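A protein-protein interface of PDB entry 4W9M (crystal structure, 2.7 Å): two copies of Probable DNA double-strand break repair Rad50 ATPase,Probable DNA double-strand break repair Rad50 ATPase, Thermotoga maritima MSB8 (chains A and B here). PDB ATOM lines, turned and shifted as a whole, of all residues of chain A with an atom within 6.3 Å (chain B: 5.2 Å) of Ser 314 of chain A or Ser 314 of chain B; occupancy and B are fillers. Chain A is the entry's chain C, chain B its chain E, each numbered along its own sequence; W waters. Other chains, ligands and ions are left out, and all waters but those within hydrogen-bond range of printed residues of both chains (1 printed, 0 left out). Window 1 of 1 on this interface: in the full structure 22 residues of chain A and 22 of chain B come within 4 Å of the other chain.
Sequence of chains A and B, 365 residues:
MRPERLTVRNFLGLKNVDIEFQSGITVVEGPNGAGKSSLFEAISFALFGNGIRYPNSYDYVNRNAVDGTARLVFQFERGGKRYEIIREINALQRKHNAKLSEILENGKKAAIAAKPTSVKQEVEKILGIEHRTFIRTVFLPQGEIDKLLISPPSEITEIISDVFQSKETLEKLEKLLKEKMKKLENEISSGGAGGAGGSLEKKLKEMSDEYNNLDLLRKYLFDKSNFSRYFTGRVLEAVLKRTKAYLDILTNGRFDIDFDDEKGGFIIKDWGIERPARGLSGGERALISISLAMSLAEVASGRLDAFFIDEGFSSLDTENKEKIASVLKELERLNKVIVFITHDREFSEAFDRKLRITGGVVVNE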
ATOM      1  N   ALA A 286       1.355 -28.417 -16.283  1.00  0.00           N
ATOM      2  CA  ALA A 286       2.040 -27.165 -16.597  1.00  0.00           C
ATOM      3  C   ALA A 286       2.202 -26.320 -15.338  1.00  0.00           C
ATOM      4  O   ALA A 286       3.224 -25.679 -15.128  1.00  0.00           O
ATOM      5  CB  ALA A 286       1.301 -26.385 -17.683  1.00  0.00           C
ATOM      6  N   GLU A 311       6.015 -20.481 -24.272  1.00  0.00           N
ATOM      7  CA  GLU A 311       4.833 -21.325 -24.392  1.00  0.00           C
ATOM      8  C   GLU A 311       4.735 -22.308 -23.229  1.00  0.00           C
ATOM      9  O   GLU A 311       5.086 -23.480 -23.363  1.00  0.00           O
ATOM     10  CB  GLU A 311       4.849 -22.084 -25.721  1.00  0.00           C
ATOM     11  CG  GLU A 311       4.106 -21.382 -26.846  1.00  0.00           C
ATOM     12  CD  GLU A 311       2.869 -20.653 -26.360  1.00  0.00           C
ATOM     13  OE1 GLU A 311       2.683 -19.477 -26.738  1.00  0.00           O
ATOM     14  OE2 GLU A 311       2.081 -21.256 -25.600  1.00  0.00           O
ATOM     15  N   GLY A 312       4.258 -21.821 -22.089  1.00  0.00           N
ATOM     16  CA  GLY A 312       4.114 -22.650 -20.907  1.00  0.00           C
ATOM     17  C   GLY A 312       2.863 -22.320 -20.115  1.00  0.00           C
ATOM     18  O   GLY A 312       2.674 -22.810 -19.003  1.00  0.00           O
ATOM     19  N   PHE A 313       2.007 -21.484 -20.693  1.00  0.00           N
ATOM     20  CA  PHE A 313       0.766 -21.084 -20.039  1.00  0.00           C
ATOM     21  C   PHE A 313      -0.406 -21.112 -21.014  1.00  0.00           C
ATOM     22  O   PHE A 313      -1.252 -20.218 -21.008  1.00  0.00           O
ATOM     23  CB  PHE A 313       0.908 -19.689 -19.427  1.00  0.00           C
ATOM     24  CG  PHE A 313       2.314 -19.340 -19.031  1.00  0.00           C
ATOM     25  CD1 PHE A 313       3.264 -19.037 -19.993  1.00  0.00           C
ATOM     26  CD2 PHE A 313       2.687 -19.316 -17.698  1.00  0.00           C
ATOM     27  CE1 PHE A 313       4.559 -18.716 -19.632  1.00  0.00           C
ATOM     28  CE2 PHE A 313       3.980 -18.996 -17.330  1.00  0.00           C
ATOM     29  CZ  PHE A 313       4.918 -18.695 -18.299  1.00  0.00           C
ATOM     30  N   SER A 314      -0.448 -22.144 -21.851  1.00  0.00           N
ATOM     31  CA  SER A 314      -1.515 -22.289 -22.834  1.00  0.00           C
ATOM     32  C   SER A 314      -2.656 -23.143 -22.289  1.00  0.00           C
ATOM     33  O   SER A 314      -3.818 -22.741 -22.326  1.00  0.00           O
ATOM     34  CB  SER A 314      -0.973 -22.901 -24.128  1.00  0.00           C
ATOM     35  OG  SER A 314      -0.363 -21.915 -24.941  1.00  0.00           O
ATOM     36  N   SER A 315      -2.314 -24.323 -21.782  1.00  0.00           N
ATOM     37  CA  SER A 315      -3.307 -25.236 -21.229  1.00  0.00           C
ATOM     38  C   SER A 315      -3.647 -24.873 -19.787  1.00  0.00           C
ATOM     39  O   SER A 315      -3.978 -25.741 -18.979  1.00  0.00           O
ATOM     40  CB  SER A 315      -2.808 -26.680 -21.303  1.00  0.00           C
ATOM     41  OG  SER A 315      -1.488 -26.739 -21.815  1.00  0.00           O
ATOM     42  N   LEU A 316      -3.562 -23.585 -19.471  1.00  0.00           N
ATOM     43  CA  LEU A 316      -3.860 -23.104 -18.126  1.00  0.00           C
ATOM     44  C   LEU A 316      -5.121 -22.246 -18.114  1.00  0.00           C
ATOM     45  O   LEU A 316      -5.152 -21.165 -18.700  1.00  0.00           O
ATOM     46  CB  LEU A 316      -2.678 -22.311 -17.567  1.00  0.00           C
ATOM     47  CG  LEU A 316      -1.487 -23.131 -17.068  1.00  0.00           C
ATOM     48  CD1 LEU A 316      -0.269 -22.243 -16.868  1.00  0.00           C
ATOM     49  CD2 LEU A 316      -1.838 -23.863 -15.782  1.00  0.00           C
ATOM     50  N   ASP A 317      -6.158 -22.736 -17.443  1.00  0.00           N
ATOM     51  CA  ASP A 317      -7.432 -22.010 -17.353  1.00  0.00           C
ATOM     52  C   ASP A 317      -7.288 -20.593 -16.731  1.00  0.00           C
ATOM     53  O   ASP A 317      -6.184 -20.181 -16.369  1.00  0.00           O
ATOM     54  CB  ASP A 317      -8.477 -22.843 -16.595  1.00  0.00           C
ATOM     55  CG  ASP A 317      -8.344 -22.763 -15.047  1.00  0.00           C
ATOM     56  OD1 ASP A 317      -7.310 -22.300 -14.507  1.00  0.00           O
ATOM     57  OD2 ASP A 317      -9.300 -23.183 -14.352  1.00  0.00           O
ATOM     58  N   HIS A 343       1.790 -15.374 -26.945  1.00  0.00           N
ATOM     59  CA  HIS A 343       1.057 -14.807 -28.059  1.00  0.00           C
ATOM     60  C   HIS A 343      -0.246 -14.299 -27.492  1.00  0.00           C
ATOM     61  O   HIS A 343      -0.968 -13.539 -28.146  1.00  0.00           O
ATOM     62  CB  HIS A 343       0.751 -15.888 -29.092  1.00  0.00           C
ATOM     63  CG  HIS A 343      -0.138 -16.958 -28.566  1.00  0.00           C
ATOM     64  ND1 HIS A 343       0.354 -18.115 -28.004  1.00  0.00           N
ATOM     65  CD2 HIS A 343      -1.484 -17.014 -28.439  1.00  0.00           C
ATOM     66  CE1 HIS A 343      -0.654 -18.857 -27.584  1.00  0.00           C
ATOM     67  NE2 HIS A 343      -1.780 -18.211 -27.831  1.00  0.00           N
ATOM     68  N   GLU B 311      -8.092 -29.909 -27.286  1.00  0.00           N
ATOM     69  CA  GLU B 311      -7.232 -28.733 -27.037  1.00  0.00           C
ATOM     70  C   GLU B 311      -6.055 -28.448 -27.990  1.00  0.00           C
ATOM     71  O   GLU B 311      -4.890 -28.506 -27.583  1.00  0.00           O
ATOM     72  CB  GLU B 311      -6.657 -28.793 -25.611  1.00  0.00           C
ATOM     73  CG  GLU B 311      -7.613 -29.259 -24.565  1.00  0.00           C
ATOM     74  CD  GLU B 311      -8.041 -28.144 -23.629  1.00  0.00           C
ATOM     75  OE1 GLU B 311      -7.949 -26.945 -24.035  1.00  0.00           O
ATOM     76  OE2 GLU B 311      -8.448 -28.485 -22.484  1.00  0.00           O
ATOM     77  N   GLY B 312      -6.320 -28.244 -29.251  1.00  0.00           N
ATOM     78  CA  GLY B 312      -5.385 -27.578 -30.129  1.00  0.00           C
ATOM     79  C   GLY B 312      -5.176 -26.090 -29.936  1.00  0.00           C
ATOM     80  O   GLY B 312      -4.098 -25.575 -29.769  1.00  0.00           O
ATOM     81  N   PHE B 313      -6.279 -25.426 -29.763  1.00  0.00           N
ATOM     82  CA  PHE B 313      -6.606 -24.150 -30.255  1.00  0.00           C
ATOM     83  C   PHE B 313      -6.048 -23.131 -29.346  1.00  0.00           C
ATOM     84  O   PHE B 313      -6.360 -22.003 -29.423  1.00  0.00           O
ATOM     85  CB  PHE B 313      -8.116 -23.965 -30.309  1.00  0.00           C
ATOM     86  CG  PHE B 313      -8.874 -25.212 -30.551  1.00  0.00           C
ATOM     87  CD1 PHE B 313      -9.271 -25.990 -29.516  1.00  0.00           C
ATOM     88  CD2 PHE B 313      -9.168 -25.598 -31.806  1.00  0.00           C
ATOM     89  CE1 PHE B 313      -9.971 -27.150 -29.736  1.00  0.00           C
ATOM     90  CE2 PHE B 313      -9.857 -26.742 -32.041  1.00  0.00           C
ATOM     91  CZ  PHE B 313     -10.248 -27.525 -31.012  1.00  0.00           C
ATOM     92  N   SER B 314      -5.271 -23.538 -28.403  1.00  0.00           N
ATOM     93  CA  SER B 314      -4.752 -22.560 -27.472  1.00  0.00           C
ATOM     94  C   SER B 314      -3.374 -22.105 -27.874  1.00  0.00           C
ATOM     95  O   SER B 314      -2.953 -21.013 -27.524  1.00  0.00           O
ATOM     96  CB  SER B 314      -4.819 -23.055 -26.031  1.00  0.00           C
ATOM     97  OG  SER B 314      -6.053 -22.637 -25.467  1.00  0.00           O
ATOM     98  N   SER B 315      -2.722 -22.848 -28.749  1.00  0.00           N
ATOM     99  CA  SER B 315      -1.488 -22.350 -29.323  1.00  0.00           C
ATOM    100  C   SER B 315      -1.831 -21.054 -30.058  1.00  0.00           C
ATOM    101  O   SER B 315      -1.020 -20.131 -30.139  1.00  0.00           O
ATOM    102  CB  SER B 315      -0.890 -23.370 -30.291  1.00  0.00           C
ATOM    103  OG  SER B 315      -0.308 -24.457 -29.592  1.00  0.00           O
ATOM    104  N   LEU B 316      -3.042 -21.016 -30.604  1.00  0.00           N
ATOM    105  CA  LEU B 316      -3.459 -20.054 -31.609  1.00  0.00           C
ATOM    106  C   LEU B 316      -3.755 -18.640 -31.039  1.00  0.00           C
ATOM    107  O   LEU B 316      -4.311 -18.519 -29.951  1.00  0.00           O
ATOM    108  CB  LEU B 316      -4.689 -20.611 -32.332  1.00  0.00           C
ATOM    109  CG  LEU B 316      -4.468 -21.779 -33.300  1.00  0.00           C
ATOM    110  CD1 LEU B 316      -5.735 -22.180 -34.064  1.00  0.00           C
ATOM    111  CD2 LEU B 316      -3.352 -21.394 -34.262  1.00  0.00           C
ATOM    112  N   LYS B 321      -7.634 -18.187 -34.011  1.00  0.00           N
ATOM    113  CA  LYS B 321      -8.563 -19.002 -33.232  1.00  0.00           C
ATOM    114  C   LYS B 321      -9.964 -18.841 -33.796  1.00  0.00           C
ATOM    115  O   LYS B 321     -10.683 -19.818 -33.986  1.00  0.00           O
ATOM    116  CB  LYS B 321      -8.529 -18.631 -31.741  1.00  0.00           C
ATOM    117  CG  LYS B 321      -8.787 -19.798 -30.819  1.00  0.00           C
ATOM    118  CD  LYS B 321      -8.818 -19.402 -29.355  1.00  0.00           C
ATOM    119  CE  LYS B 321      -7.452 -18.980 -28.825  1.00  0.00           C
ATOM    120  NZ  LYS B 321      -7.016 -19.825 -27.657  1.00  0.00           N
ATOM    121  N   HIS B 343     -10.914 -25.526 -22.393  1.00  0.00           N
ATOM    122  CA  HIS B 343     -11.184 -24.735 -21.192  1.00  0.00           C
ATOM    123  C   HIS B 343     -11.436 -23.279 -21.609  1.00  0.00           C
ATOM    124  O   HIS B 343     -12.149 -22.535 -20.924  1.00  0.00           O
ATOM    125  CB  HIS B 343     -10.004 -24.805 -20.230  1.00  0.00           C
ATOM    126  CG  HIS B 343      -8.721 -24.308 -20.821  1.00  0.00           C
ATOM    127  ND1 HIS B 343      -7.767 -25.154 -21.351  1.00  0.00           N
ATOM    128  CD2 HIS B 343      -8.245 -23.049 -20.985  1.00  0.00           C
ATOM    129  CE1 HIS B 343      -6.757 -24.435 -21.813  1.00  0.00           C
ATOM    130  NE2 HIS B 343      -7.024 -23.155 -21.605  1.00  0.00           N
ATOM    131  N   ASP B 344     -10.852 -22.906 -22.750  1.00  0.00           N
ATOM    132  CA  ASP B 344     -10.975 -21.593 -23.388  1.00  0.00           C
ATOM    133  C   ASP B 344     -12.406 -21.210 -23.736  1.00  0.00           C
ATOM    134  O   ASP B 344     -12.979 -21.768 -24.657  1.00  0.00           O
ATOM    135  CB  ASP B 344     -10.182 -21.647 -24.693  1.00  0.00           C
ATOM    136  CG  ASP B 344      -9.925 -20.273 -25.310  1.00  0.00           C
ATOM    137  OD1 ASP B 344     -10.669 -19.292 -25.021  1.00  0.00           O
ATOM    138  OD2 ASP B 344      -8.953 -20.205 -26.108  1.00  0.00           O
HETATM  139  O   HOH W   1       1.266 -20.824 -29.829  1.00  0.00           O
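Of the 9 printed residues of chain B, 4 touch a printed residue of chain A.
Of the 9 printed residues of chain A, 5 touch a printed residue of chain B.
Hydrophobic or aromatic side chains of chain A within 4 Å of the printed part of chain B: His 343.
Among the printed residues, 8 pairs touch across the chains.
Among the printed residues, no Asp or Glu carboxylate lies within 4 Å of a Lys or Arg side-chain nitrogen of the other chain.
O of Ser 314 of chain B is in hydrogen-bond range of NE2 of His 343 of chain A (3.1 Å).
The backbone carbonyl oxygen (O) of Ser 314 of chain A sits at hydrogen-bond distance from a ring nitrogen (NE2) of His 343 of chain B.
NE2 of His 343 of chain A is in hydrogen-bond range of O of Leu 316 of chain B, 3.3 Å away.
NE2 of His 343 of chain A lies close to O of Ser 315 of chain B (3.1 Å).
Water W1 bridges the backbone carbonyl oxygen (O) of Ser 315 of chain B (2.4 Å) and a ring nitrogen (ND1) of His 343 of chain A (3.4 Å).
Ser 314 of chain A touches two residues of chain B.
Of the printed residues of chain B, Leu 316 of chain A touches His 343 (3.99 Å).
Of the printed residues of chain B, Asp 317 of chain A touches His 343.
Printed residues of chain B within 4 Å of His 343 of chain A: Ser 314, Ser 315 and Leu 316.
Glu 311 of chain B touches none of the printed residues of chain A.
Of the printed residues of chain A, Leu 316 of chain B touches His 343.
Lys 321 of chain B touches none of the printed residues of chain A.
The nearest residue of chain B that does not touch Ser 314 of chain A is Ser 315 of chain B (4.5 Å).
The nearest printed residue of chain A that does not touch Leu 316 of chain B is Ser 314 of chain A (6.3 Å).
Ser 314 of chain A touches Ser 314 of chain B.
CE1 of His 343 of chain B touches CA of Ser 315 of chain A, 3.6 Å away.
O of Leu 316 of chain A touches NE2 of His 343 of chain B (3.99 Å).
CA of Asp 317 of chain A touches CD2 of His 343 of chain B, 3.9 Å away.
Ser 314 of chain A touches its own counterpart, Ser 314 of chain B.
Ser 314 of chain A touches His 343 of chain B, and with the chains exchanged His 343 of chain A touches Ser 314 of chain B.
Ser 315 of chain A touches His 343 of chain B, and with the chains exchanged His 343 of chain A touches Ser 315 of chain B.
Leu 316 of chain A touches His 343 of chain B, and with the chains exchanged His 343 of chain A touches Leu 316 of chain B.
7 positions are printed for both chains.
The side-chain carboxylate (OE1) of Glu 311 of chain A is in hydrogen-bond range of a ring nitrogen (ND1) of His 343 of chain A.
OE2 of Glu 311 of chain A is in hydrogen-bond range of OG of Ser 314 of chain A (2.6 Å).
The side-chain carboxylate (OE1) of Glu 311 of chain B is in hydrogen-bond range of a ring nitrogen (ND1) of His 343 of chain B, 3.2 Å away.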
